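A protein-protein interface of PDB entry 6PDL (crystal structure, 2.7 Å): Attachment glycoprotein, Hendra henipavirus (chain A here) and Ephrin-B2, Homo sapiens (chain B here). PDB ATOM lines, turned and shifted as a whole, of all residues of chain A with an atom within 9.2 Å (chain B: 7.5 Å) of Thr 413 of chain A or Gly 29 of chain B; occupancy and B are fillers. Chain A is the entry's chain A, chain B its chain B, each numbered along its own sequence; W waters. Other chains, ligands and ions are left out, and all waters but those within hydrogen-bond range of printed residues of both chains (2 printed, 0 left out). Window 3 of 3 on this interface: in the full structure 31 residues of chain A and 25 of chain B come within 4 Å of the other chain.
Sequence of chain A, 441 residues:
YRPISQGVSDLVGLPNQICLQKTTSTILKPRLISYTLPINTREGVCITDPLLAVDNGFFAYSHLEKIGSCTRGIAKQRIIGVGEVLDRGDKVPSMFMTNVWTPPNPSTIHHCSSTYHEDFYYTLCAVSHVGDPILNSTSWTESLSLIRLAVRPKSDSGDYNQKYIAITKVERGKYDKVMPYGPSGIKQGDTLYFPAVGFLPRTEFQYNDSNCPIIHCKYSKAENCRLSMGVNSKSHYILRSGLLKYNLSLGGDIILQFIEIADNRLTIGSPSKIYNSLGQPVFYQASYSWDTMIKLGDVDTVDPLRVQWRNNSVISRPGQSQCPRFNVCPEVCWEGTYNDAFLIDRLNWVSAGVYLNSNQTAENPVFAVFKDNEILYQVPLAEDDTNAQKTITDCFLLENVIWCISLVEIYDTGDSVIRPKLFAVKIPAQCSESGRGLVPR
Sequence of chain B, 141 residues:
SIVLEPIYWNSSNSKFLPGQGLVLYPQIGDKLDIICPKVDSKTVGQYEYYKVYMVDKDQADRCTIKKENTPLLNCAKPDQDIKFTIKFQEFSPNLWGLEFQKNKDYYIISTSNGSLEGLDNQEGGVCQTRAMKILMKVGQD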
ATOM      1  N   THR A 361      -6.322 -22.469 -33.276  1.00  0.00           N
ATOM      2  CA  THR A 361      -5.561 -23.571 -32.708  1.00  0.00           C
ATOM      3  C   THR A 361      -6.235 -24.896 -33.041  1.00  0.00           C
ATOM      4  O   THR A 361      -7.456 -24.970 -33.209  1.00  0.00           O
ATOM      5  CB  THR A 361      -5.402 -23.426 -31.193  1.00  0.00           C
ATOM      6  OG1 THR A 361      -6.676 -23.143 -30.606  1.00  0.00           O
ATOM      7  CG2 THR A 361      -4.441 -22.300 -30.868  1.00  0.00           C
ATOM      8  N   ALA A 362      -5.422 -25.943 -33.156  1.00  0.00           N
ATOM      9  CA  ALA A 362      -5.917 -27.292 -33.435  1.00  0.00           C
ATOM     10  C   ALA A 362      -6.268 -27.999 -32.125  1.00  0.00           C
ATOM     11  O   ALA A 362      -5.514 -28.824 -31.605  1.00  0.00           O
ATOM     12  CB  ALA A 362      -4.877 -28.066 -34.236  1.00  0.00           C
ATOM     13  N   GLU A 363      -7.443 -27.673 -31.580  1.00  0.00           N
ATOM     14  CA  GLU A 363      -7.877 -28.321 -30.347  1.00  0.00           C
ATOM     15  C   GLU A 363      -9.396 -28.262 -30.214  1.00  0.00           C
ATOM     16  O   GLU A 363     -10.086 -27.587 -30.983  1.00  0.00           O
ATOM     17  CB  GLU A 363      -7.176 -27.709 -29.121  1.00  0.00           C
ATOM     18  CG  GLU A 363      -7.456 -26.243 -28.821  1.00  0.00           C
ATOM     19  CD  GLU A 363      -6.638 -25.739 -27.633  1.00  0.00           C
ATOM     20  OE1 GLU A 363      -5.843 -26.534 -27.081  1.00  0.00           O
ATOM     21  OE2 GLU A 363      -6.798 -24.558 -27.242  1.00  0.00           O
ATOM     22  N   ASP A 384     -11.754 -29.719 -23.412  1.00  0.00           N
ATOM     23  CA  ASP A 384     -11.240 -28.590 -24.145  1.00  0.00           C
ATOM     24  C   ASP A 384      -9.727 -28.659 -24.043  1.00  0.00           C
ATOM     25  O   ASP A 384      -9.177 -29.490 -23.315  1.00  0.00           O
ATOM     26  CB  ASP A 384     -11.750 -27.273 -23.555  1.00  0.00           C
ATOM     27  CG  ASP A 384     -13.223 -27.299 -23.238  1.00  0.00           C
ATOM     28  OD1 ASP A 384     -13.935 -26.366 -23.663  1.00  0.00           O
ATOM     29  OD2 ASP A 384     -13.656 -28.213 -22.490  1.00  0.00           O
ATOM     30  N   ASP A 385      -9.054 -27.844 -24.844  1.00  0.00           N
ATOM     31  CA  ASP A 385      -7.602 -27.805 -24.833  1.00  0.00           C
ATOM     32  C   ASP A 385      -7.029 -29.207 -25.059  1.00  0.00           C
ATOM     33  O   ASP A 385      -5.836 -29.422 -24.839  1.00  0.00           O
ATOM     34  CB  ASP A 385      -7.063 -27.125 -23.549  1.00  0.00           C
ATOM     35  CG  ASP A 385      -7.170 -27.994 -22.300  1.00  0.00           C
ATOM     36  OD1 ASP A 385      -6.438 -28.996 -22.188  1.00  0.00           O
ATOM     37  OD2 ASP A 385      -8.001 -27.666 -21.423  1.00  0.00           O
ATOM     38  N   THR A 386      -7.867 -30.178 -25.442  1.00  0.00           N
ATOM     39  CA  THR A 386      -7.368 -31.433 -25.982  1.00  0.00           C
ATOM     40  C   THR A 386      -6.949 -31.156 -27.418  1.00  0.00           C
ATOM     41  O   THR A 386      -7.722 -30.575 -28.186  1.00  0.00           O
ATOM     42  CB  THR A 386      -8.426 -32.537 -25.940  1.00  0.00           C
ATOM     43  OG1 THR A 386      -8.887 -32.727 -24.595  1.00  0.00           O
ATOM     44  CG2 THR A 386      -7.861 -33.852 -26.471  1.00  0.00           C
ATOM     45  N   ASN A 387      -5.753 -31.593 -27.794  1.00  0.00           N
ATOM     46  CA  ASN A 387      -5.230 -31.282 -29.117  1.00  0.00           C
ATOM     47  C   ASN A 387      -5.838 -32.214 -30.158  1.00  0.00           C
ATOM     48  O   ASN A 387      -5.909 -33.429 -29.950  1.00  0.00           O
ATOM     49  CB  ASN A 387      -3.707 -31.380 -29.116  1.00  0.00           C
ATOM     50  CG  ASN A 387      -3.075 -30.538 -28.018  1.00  0.00           C
ATOM     51  OD1 ASN A 387      -3.528 -29.429 -27.734  1.00  0.00           O
ATOM     52  ND2 ASN A 387      -2.029 -31.063 -27.393  1.00  0.00           N
ATOM     53  N   ALA A 388      -6.289 -31.638 -31.270  1.00  0.00           N
ATOM     54  CA  ALA A 388      -6.912 -32.412 -32.332  1.00  0.00           C
ATOM     55  C   ALA A 388      -6.638 -31.756 -33.677  1.00  0.00           C
ATOM     56  O   ALA A 388      -6.434 -30.546 -33.768  1.00  0.00           O
ATOM     57  CB  ALA A 388      -8.419 -32.572 -32.101  1.00  0.00           C
ATOM     58  N   ILE A 410      -5.659 -36.912 -32.438  1.00  0.00           N
ATOM     59  CA  ILE A 410      -5.971 -36.411 -31.106  1.00  0.00           C
ATOM     60  C   ILE A 410      -4.836 -36.776 -30.163  1.00  0.00           C
ATOM     61  O   ILE A 410      -4.137 -37.772 -30.365  1.00  0.00           O
ATOM     62  CB  ILE A 410      -7.322 -36.979 -30.612  1.00  0.00           C
ATOM     63  CG1 ILE A 410      -8.000 -36.025 -29.631  1.00  0.00           C
ATOM     64  CG2 ILE A 410      -7.125 -38.328 -29.976  1.00  0.00           C
ATOM     65  CD1 ILE A 410      -9.452 -36.375 -29.374  1.00  0.00           C
ATOM     66  N   TYR A 411      -4.617 -35.929 -29.160  1.00  0.00           N
ATOM     67  CA  TYR A 411      -3.745 -36.272 -28.045  1.00  0.00           C
ATOM     68  C   TYR A 411      -3.873 -35.200 -26.977  1.00  0.00           C
ATOM     69  O   TYR A 411      -4.180 -34.042 -27.274  1.00  0.00           O
ATOM     70  CB  TYR A 411      -2.279 -36.445 -28.478  1.00  0.00           C
ATOM     71  CG  TYR A 411      -1.405 -35.203 -28.548  1.00  0.00           C
ATOM     72  CD1 TYR A 411      -0.639 -34.804 -27.459  1.00  0.00           C
ATOM     73  CD2 TYR A 411      -1.292 -34.474 -29.724  1.00  0.00           C
ATOM     74  CE1 TYR A 411       0.180 -33.694 -27.525  1.00  0.00           C
ATOM     75  CE2 TYR A 411      -0.471 -33.360 -29.800  1.00  0.00           C
ATOM     76  CZ  TYR A 411       0.265 -32.976 -28.698  1.00  0.00           C
ATOM     77  OH  TYR A 411       1.084 -31.868 -28.768  1.00  0.00           O
ATOM     78  N   ASP A 412      -3.638 -35.609 -25.735  1.00  0.00           N
ATOM     79  CA  ASP A 412      -3.643 -34.710 -24.591  1.00  0.00           C
ATOM     80  C   ASP A 412      -2.205 -34.371 -24.225  1.00  0.00           C
ATOM     81  O   ASP A 412      -1.319 -35.226 -24.312  1.00  0.00           O
ATOM     82  CB  ASP A 412      -4.366 -35.346 -23.404  1.00  0.00           C
ATOM     83  CG  ASP A 412      -5.843 -34.992 -23.365  1.00  0.00           C
ATOM     84  OD1 ASP A 412      -6.159 -33.788 -23.274  1.00  0.00           O
ATOM     85  OD2 ASP A 412      -6.688 -35.912 -23.427  1.00  0.00           O
ATOM     86  N   THR A 413      -1.977 -33.117 -23.831  1.00  0.00           N
ATOM     87  CA  THR A 413      -0.622 -32.665 -23.534  1.00  0.00           C
ATOM     88  C   THR A 413       0.018 -33.564 -22.478  1.00  0.00           C
ATOM     89  O   THR A 413      -0.560 -33.808 -21.416  1.00  0.00           O
ATOM     90  CB  THR A 413      -0.653 -31.210 -23.056  1.00  0.00           C
ATOM     91  OG1 THR A 413      -0.925 -30.342 -24.166  1.00  0.00           O
ATOM     92  CG2 THR A 413       0.677 -30.815 -22.427  1.00  0.00           C
ATOM     93  N   GLY A 414       1.221 -34.056 -22.777  1.00  0.00           N
ATOM     94  CA  GLY A 414       1.904 -35.001 -21.922  1.00  0.00           C
ATOM     95  C   GLY A 414       1.818 -36.462 -22.324  1.00  0.00           C
ATOM     96  O   GLY A 414       2.472 -37.292 -21.688  1.00  0.00           O
ATOM     97  N   ASP A 415       1.046 -36.805 -23.348  1.00  0.00           N
ATOM     98  CA  ASP A 415       0.968 -38.187 -23.814  1.00  0.00           C
ATOM     99  C   ASP A 415       2.328 -38.646 -24.355  1.00  0.00           C
ATOM    100  O   ASP A 415       3.078 -37.855 -24.923  1.00  0.00           O
ATOM    101  CB  ASP A 415      -0.119 -38.310 -24.887  1.00  0.00           C
ATOM    102  CG  ASP A 415      -1.544 -38.328 -24.310  1.00  0.00           C
ATOM    103  OD1 ASP A 415      -2.515 -38.488 -25.087  1.00  0.00           O
ATOM    104  OD2 ASP A 415      -1.683 -38.194 -23.073  1.00  0.00           O
ATOM    105  N   SER A 416       2.652 -39.942 -24.196  1.00  0.00           N
ATOM    106  CA  SER A 416       3.946 -40.431 -24.686  1.00  0.00           C
ATOM    107  C   SER A 416       3.896 -40.536 -26.180  1.00  0.00           C
ATOM    108  O   SER A 416       4.905 -40.404 -26.891  1.00  0.00           O
ATOM    109  CB  SER A 416       4.174 -41.908 -24.415  1.00  0.00           C
ATOM    110  OG  SER A 416       3.636 -42.355 -23.167  1.00  0.00           O
ATOM    111  N   VAL A 417       2.716 -40.928 -26.619  1.00  0.00           N
ATOM    112  CA  VAL A 417       2.439 -41.390 -27.962  1.00  0.00           C
ATOM    113  C   VAL A 417       1.299 -40.546 -28.478  1.00  0.00           C
ATOM    114  O   VAL A 417       0.263 -40.408 -27.816  1.00  0.00           O
ATOM    115  CB  VAL A 417       2.046 -42.880 -27.974  1.00  0.00           C
ATOM    116  CG1 VAL A 417       1.448 -43.265 -29.304  1.00  0.00           C
ATOM    117  CG2 VAL A 417       3.245 -43.760 -27.625  1.00  0.00           C
ATOM    118  N   ILE A 418       1.482 -40.015 -29.670  1.00  0.00           N
ATOM    119  CA  ILE A 418       0.437 -39.297 -30.378  1.00  0.00           C
ATOM    120  C   ILE A 418      -0.179 -40.299 -31.334  1.00  0.00           C
ATOM    121  O   ILE A 418       0.513 -40.874 -32.187  1.00  0.00           O
ATOM    122  CB  ILE A 418       1.001 -38.062 -31.087  1.00  0.00           C
ATOM    123  CG1 ILE A 418       1.259 -36.971 -30.043  1.00  0.00           C
ATOM    124  CG2 ILE A 418       0.056 -37.578 -32.154  1.00  0.00           C
ATOM    125  CD1 ILE A 418       2.356 -35.997 -30.410  1.00  0.00           C
ATOM    126  N   SER B   1      -0.107 -24.981 -17.761  1.00  0.00           N
ATOM    127  CA  SER B   1      -1.488 -25.304 -17.881  1.00  0.00           C
ATOM    128  C   SER B   1      -2.043 -24.016 -18.315  1.00  0.00           C
ATOM    129  O   SER B   1      -3.203 -23.775 -18.035  1.00  0.00           O
ATOM    130  CB  SER B   1      -2.121 -25.489 -16.538  1.00  0.00           C
ATOM    131  OG  SER B   1      -1.275 -26.297 -15.722  1.00  0.00           O
ATOM    132  N   ILE B   2      -1.230 -23.121 -18.846  1.00  0.00           N
ATOM    133  CA  ILE B   2      -1.571 -21.723 -18.698  1.00  0.00           C
ATOM    134  C   ILE B   2      -1.754 -21.077 -20.061  1.00  0.00           C
ATOM    135  O   ILE B   2      -1.207 -21.513 -21.072  1.00  0.00           O
ATOM    136  CB  ILE B   2      -0.496 -20.941 -17.868  1.00  0.00           C
ATOM    137  CG1 ILE B   2      -0.240 -21.576 -16.487  1.00  0.00           C
ATOM    138  CG2 ILE B   2      -0.883 -19.461 -17.658  1.00  0.00           C
ATOM    139  CD1 ILE B   2       0.532 -20.618 -15.556  1.00  0.00           C
ATOM    140  N   VAL B   3      -2.539 -19.999 -20.056  1.00  0.00           N
ATOM    141  CA  VAL B   3      -2.554 -19.029 -21.142  1.00  0.00           C
ATOM    142  C   VAL B   3      -1.540 -17.933 -20.811  1.00  0.00           C
ATOM    143  O   VAL B   3      -1.685 -17.228 -19.803  1.00  0.00           O
ATOM    144  CB  VAL B   3      -3.958 -18.430 -21.326  1.00  0.00           C
ATOM    145  CG1 VAL B   3      -3.880 -17.056 -21.991  1.00  0.00           C
ATOM    146  CG2 VAL B   3      -4.839 -19.336 -22.151  1.00  0.00           C
ATOM    147  N   PRO B  26       8.093 -20.111 -22.931  1.00  0.00           N
ATOM    148  CA  PRO B  26       6.824 -20.846 -22.855  1.00  0.00           C
ATOM    149  C   PRO B  26       7.045 -22.353 -22.787  1.00  0.00           C
ATOM    150  O   PRO B  26       8.029 -22.887 -23.300  1.00  0.00           O
ATOM    151  CB  PRO B  26       6.101 -20.443 -24.145  1.00  0.00           C
ATOM    152  CG  PRO B  26       7.178 -20.101 -25.096  1.00  0.00           C
ATOM    153  CD  PRO B  26       8.400 -19.694 -24.312  1.00  0.00           C
ATOM    154  N   GLN B  27       6.121 -23.042 -22.127  1.00  0.00           N
ATOM    155  CA  GLN B  27       6.206 -24.489 -21.963  1.00  0.00           C
ATOM    156  C   GLN B  27       5.201 -25.191 -22.873  1.00  0.00           C
ATOM    157  O   GLN B  27       4.265 -24.575 -23.393  1.00  0.00           O
ATOM    158  CB  GLN B  27       5.994 -24.892 -20.498  1.00  0.00           C
ATOM    159  CG  GLN B  27       7.158 -24.503 -19.575  1.00  0.00           C
ATOM    160  CD  GLN B  27       8.234 -25.575 -19.496  1.00  0.00           C
ATOM    161  OE1 GLN B  27       8.053 -26.687 -19.993  1.00  0.00           O
ATOM    162  NE2 GLN B  27       9.368 -25.238 -18.886  1.00  0.00           N
ATOM    163  N   ILE B  28       5.439 -26.483 -23.117  1.00  0.00           N
ATOM    164  CA  ILE B  28       4.545 -27.251 -23.980  1.00  0.00           C
ATOM    165  C   ILE B  28       3.139 -27.244 -23.397  1.00  0.00           C
ATOM    166  O   ILE B  28       2.938 -27.512 -22.206  1.00  0.00           O
ATOM    167  CB  ILE B  28       5.063 -28.686 -24.157  1.00  0.00           C
ATOM    168  CG1 ILE B  28       6.349 -28.693 -24.985  1.00  0.00           C
ATOM    169  CG2 ILE B  28       4.010 -29.551 -24.827  1.00  0.00           C
ATOM    170  CD1 ILE B  28       6.279 -27.838 -26.226  1.00  0.00           C
ATOM    171  N   GLY B  29       2.152 -26.953 -24.243  1.00  0.00           N
ATOM    172  CA  GLY B  29       0.773 -26.851 -23.820  1.00  0.00           C
ATOM    173  C   GLY B  29       0.279 -25.440 -23.585  1.00  0.00           C
ATOM    174  O   GLY B  29      -0.933 -25.249 -23.425  1.00  0.00           O
ATOM    175  N   ASP B  30       1.162 -24.445 -23.594  1.00  0.00           N
ATOM    176  CA  ASP B  30       0.717 -23.085 -23.342  1.00  0.00           C
ATOM    177  C   ASP B  30       0.064 -22.498 -24.587  1.00  0.00           C
ATOM    178  O   ASP B  30       0.215 -23.006 -25.702  1.00  0.00           O
ATOM    179  CB  ASP B  30       1.892 -22.193 -22.930  1.00  0.00           C
ATOM    180  CG  ASP B  30       2.502 -22.590 -21.602  1.00  0.00           C
ATOM    181  OD1 ASP B  30       2.894 -23.760 -21.442  1.00  0.00           O
ATOM    182  OD2 ASP B  30       2.607 -21.718 -20.715  1.00  0.00           O
ATOM    183  N   LYS B  31      -0.676 -21.413 -24.382  1.00  0.00           N
ATOM    184  CA  LYS B  31      -1.282 -20.665 -25.470  1.00  0.00           C
ATOM    185  C   LYS B  31      -0.803 -19.221 -25.403  1.00  0.00           C
ATOM    186  O   LYS B  31      -0.602 -18.676 -24.314  1.00  0.00           O
ATOM    187  CB  LYS B  31      -2.809 -20.733 -25.406  1.00  0.00           C
ATOM    188  CG  LYS B  31      -3.384 -21.885 -26.205  1.00  0.00           C
ATOM    189  CD  LYS B  31      -4.791 -22.232 -25.759  1.00  0.00           C
ATOM    190  CE  LYS B  31      -5.800 -21.211 -26.253  1.00  0.00           C
ATOM    191  NZ  LYS B  31      -7.185 -21.528 -25.780  1.00  0.00           N
ATOM    192  N   LEU B  32      -0.606 -18.604 -26.565  1.00  0.00           N
ATOM    193  CA  LEU B  32      -0.126 -17.231 -26.612  1.00  0.00           C
ATOM    194  C   LEU B  32      -0.822 -16.465 -27.725  1.00  0.00           C
ATOM    195  O   LEU B  32      -1.030 -16.994 -28.819  1.00  0.00           O
ATOM    196  CB  LEU B  32       1.391 -17.176 -26.821  1.00  0.00           C
ATOM    197  CG  LEU B  32       1.969 -15.763 -26.881  1.00  0.00           C
ATOM    198  CD1 LEU B  32       1.727 -15.029 -25.573  1.00  0.00           C
ATOM    199  CD2 LEU B  32       3.436 -15.810 -27.202  1.00  0.00           C
ATOM    200  N   ILE B  86      -1.000 -18.929 -30.742  1.00  0.00           N
ATOM    201  CA  ILE B  86      -0.177 -20.123 -30.818  1.00  0.00           C
ATOM    202  C   ILE B  86      -0.547 -21.010 -29.645  1.00  0.00           C
ATOM    203  O   ILE B  86      -0.727 -20.525 -28.525  1.00  0.00           O
ATOM    204  CB  ILE B  86       1.330 -19.810 -30.774  1.00  0.00           C
ATOM    205  CG1 ILE B  86       1.735 -18.803 -31.843  1.00  0.00           C
ATOM    206  CG2 ILE B  86       2.121 -21.083 -30.925  1.00  0.00           C
ATOM    207  CD1 ILE B  86       3.189 -18.376 -31.728  1.00  0.00           C
ATOM    208  N   LYS B  87      -0.687 -22.298 -29.906  1.00  0.00           N
ATOM    209  CA  LYS B  87      -0.595 -23.299 -28.860  1.00  0.00           C
ATOM    210  C   LYS B  87       0.673 -24.083 -29.134  1.00  0.00           C
ATOM    211  O   LYS B  87       0.916 -24.501 -30.273  1.00  0.00           O
ATOM    212  CB  LYS B  87      -1.810 -24.227 -28.813  1.00  0.00           C
ATOM    213  CG  LYS B  87      -1.634 -25.335 -27.778  1.00  0.00           C
ATOM    214  CD  LYS B  87      -2.938 -25.798 -27.185  1.00  0.00           C
ATOM    215  CE  LYS B  87      -2.700 -26.841 -26.104  1.00  0.00           C
ATOM    216  NZ  LYS B  87      -3.876 -27.722 -25.898  1.00  0.00           N
ATOM    217  N   PHE B  88       1.496 -24.245 -28.104  1.00  0.00           N
ATOM    218  CA  PHE B  88       2.803 -24.871 -28.260  1.00  0.00           C
ATOM    219  C   PHE B  88       2.616 -26.382 -28.201  1.00  0.00           C
ATOM    220  O   PHE B  88       2.823 -27.038 -27.176  1.00  0.00           O
ATOM    221  CB  PHE B  88       3.760 -24.351 -27.201  1.00  0.00           C
ATOM    222  CG  PHE B  88       4.091 -22.899 -27.365  1.00  0.00           C
ATOM    223  CD1 PHE B  88       3.360 -21.926 -26.699  1.00  0.00           C
ATOM    224  CD2 PHE B  88       5.120 -22.504 -28.204  1.00  0.00           C
ATOM    225  CE1 PHE B  88       3.660 -20.588 -26.856  1.00  0.00           C
ATOM    226  CE2 PHE B  88       5.428 -21.168 -28.368  1.00  0.00           C
ATOM    227  CZ  PHE B  88       4.696 -20.206 -27.693  1.00  0.00           C
ATOM    228  N   GLN B  89       2.195 -26.935 -29.335  1.00  0.00           N
ATOM    229  CA  GLN B  89       1.862 -28.344 -29.455  1.00  0.00           C
ATOM    230  C   GLN B  89       2.275 -28.834 -30.834  1.00  0.00           C
ATOM    231  O   GLN B  89       2.797 -28.077 -31.658  1.00  0.00           O
ATOM    232  CB  GLN B  89       0.371 -28.578 -29.225  1.00  0.00           C
ATOM    233  CG  GLN B  89      -0.507 -27.732 -30.116  1.00  0.00           C
ATOM    234  CD  GLN B  89      -1.729 -28.488 -30.587  1.00  0.00           C
ATOM    235  OE1 GLN B  89      -1.667 -29.695 -30.824  1.00  0.00           O
ATOM    236  NE2 GLN B  89      -2.854 -27.787 -30.714  1.00  0.00           N
ATOM    237  N   PHE B 100       6.553 -26.498 -32.248  1.00  0.00           N
ATOM    238  CA  PHE B 100       7.321 -26.068 -31.099  1.00  0.00           C
ATOM    239  C   PHE B 100       7.666 -27.276 -30.231  1.00  0.00           C
ATOM    240  O   PHE B 100       6.785 -27.956 -29.690  1.00  0.00           O
ATOM    241  CB  PHE B 100       6.554 -24.992 -30.372  1.00  0.00           C
ATOM    242  CG  PHE B 100       6.227 -23.832 -31.269  1.00  0.00           C
ATOM    243  CD1 PHE B 100       4.918 -23.568 -31.622  1.00  0.00           C
ATOM    244  CD2 PHE B 100       7.236 -23.045 -31.809  1.00  0.00           C
ATOM    245  CE1 PHE B 100       4.618 -22.511 -32.468  1.00  0.00           C
ATOM    246  CE2 PHE B 100       6.935 -21.983 -32.650  1.00  0.00           C
ATOM    247  CZ  PHE B 100       5.625 -21.715 -32.975  1.00  0.00           C
ATOM    248  N   VAL B 138      11.363 -22.622 -25.484  1.00  0.00           N
ATOM    249  CA  VAL B 138      10.224 -23.500 -25.245  1.00  0.00           C
ATOM    250  C   VAL B 138      10.624 -24.617 -24.289  1.00  0.00           C
ATOM    251  O   VAL B 138      11.622 -25.315 -24.505  1.00  0.00           O
ATOM    252  CB  VAL B 138       9.668 -24.045 -26.567  1.00  0.00           C
ATOM    253  CG1 VAL B 138       8.439 -24.901 -26.315  1.00  0.00           C
ATOM    254  CG2 VAL B 138       9.295 -22.887 -27.454  1.00  0.00           C
HETATM  255  O   HOH W   1      -2.494 -25.688 -32.523  1.00  0.00           O
HETATM  256  O   HOH W   2      -9.049 -22.766 -27.875  1.00  0.00           O
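O of Ala 362 of chain A is in hydrogen-bond range of NE2 of Gln 89 of chain B.
OE2 of Glu 363 of chain A is in salt-bridge range of NZ of Lys 31 of chain B.
NZ of Lys 87 of chain B lies within salt-bridge range of OE1 of Glu 363 of chain A, 2.6 Å away.
The backbone carbonyl oxygen (O) of Asp 385 of chain A lies within hydrogen-bond range of the side-chain amino group (NZ) of Lys 87 of chain B, 2.8 Å away.
The side-chain amino group of Lys 87 of chain B is in hydrogen-bond range of the side-chain amide oxygen of Asn 387 of chain A, 2.5 Å away.
The side-chain amide oxygen of Asn 387 of chain A lies within hydrogen-bond range of the side-chain amide nitrogen of Gln 89 of chain B.
N of Ala 388 of chain A is in hydrogen-bond range of O of Ala 362 of chain A.
The backbone carbonyl oxygen (O) of Asn 387 of chain A sits at hydrogen-bond distance from the backbone NH (N) of Tyr 411 of chain A.
The side-chain amide nitrogen (ND2) of Asn 387 of chain A lies within hydrogen-bond range of the side-chain hydroxyl (OG1) of Thr 413 of chain A.
The backbone carbonyl oxygen of Ile 2 of chain B is in hydrogen-bond range of the backbone NH of Lys 31 of chain B (3.4 Å).
N of Gly 29 of chain B sits at hydrogen-bond distance from O of Phe 88 of chain B (3.0 Å).
Among the printed residues, merely in contact across the chains: Thr 361 of chain A with Lys 87 of chain B (3.9 Å), Tyr 411 of chain A with Gln 89 of chain B (3.4 Å) and Thr 413 of chain A with Gly 29 of chain B (3.9 Å).
Of the printed residues of chain B, Thr 413 of chain A touches Gly 29 (3.9 Å).
Of chain A, only Thr 413 (3.9 Å) comes within 4 Å of Gly 29 of chain B.
Printed residues of chain A within 4 Å of Lys 31 of chain B: Glu 363 (3.4 Å).
Printed residues of chain B within 4 Å of Glu 363 of chain A: Lys 31 (3.4 Å) and Lys 87 (2.6 Å).
Printed residues of chain B within 4 Å of Asn 387 of chain A: Lys 87 (2.5 Å) and Gln 89 (3.1 Å).
Of the printed residues of chain A, Gln 89 of chain B touches Ala 362, Asn 387 and Tyr 411.
Of the printed residues of chain B, Thr 361 of chain A touches Lys 87.
Val 417 of chain A touches none of the printed residues of chain B.
Ile 28 of chain B touches none of the printed residues of chain A.
The nearest printed residue of chain B that does not touch Thr 413 of chain A is Ile 28 of chain B (4.01 Å).
The nearest residue of chain A that does not touch Gly 29 of chain B is Asn 387 of chain A (6.2 Å).
Of the 16 printed residues of chain B, 4 touch a printed residue of chain A.
Printed residues of chain A that touch a printed residue of chain B: Thr 361, Ala 362, Glu 363, Asp 385, Asn 387, Tyr 411 and Thr 413.
Among the printed residues, 9 pairs touch across the chains.
Water W1 lies within hydrogen-bond range of NE2 of Gln 89 of chain B (2.8 Å) and N of Ala 362 of chain A (3.0 Å).
Water W2 bridges OE2 of Glu 363 of chain A and NZ of Lys 31 of chain B.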
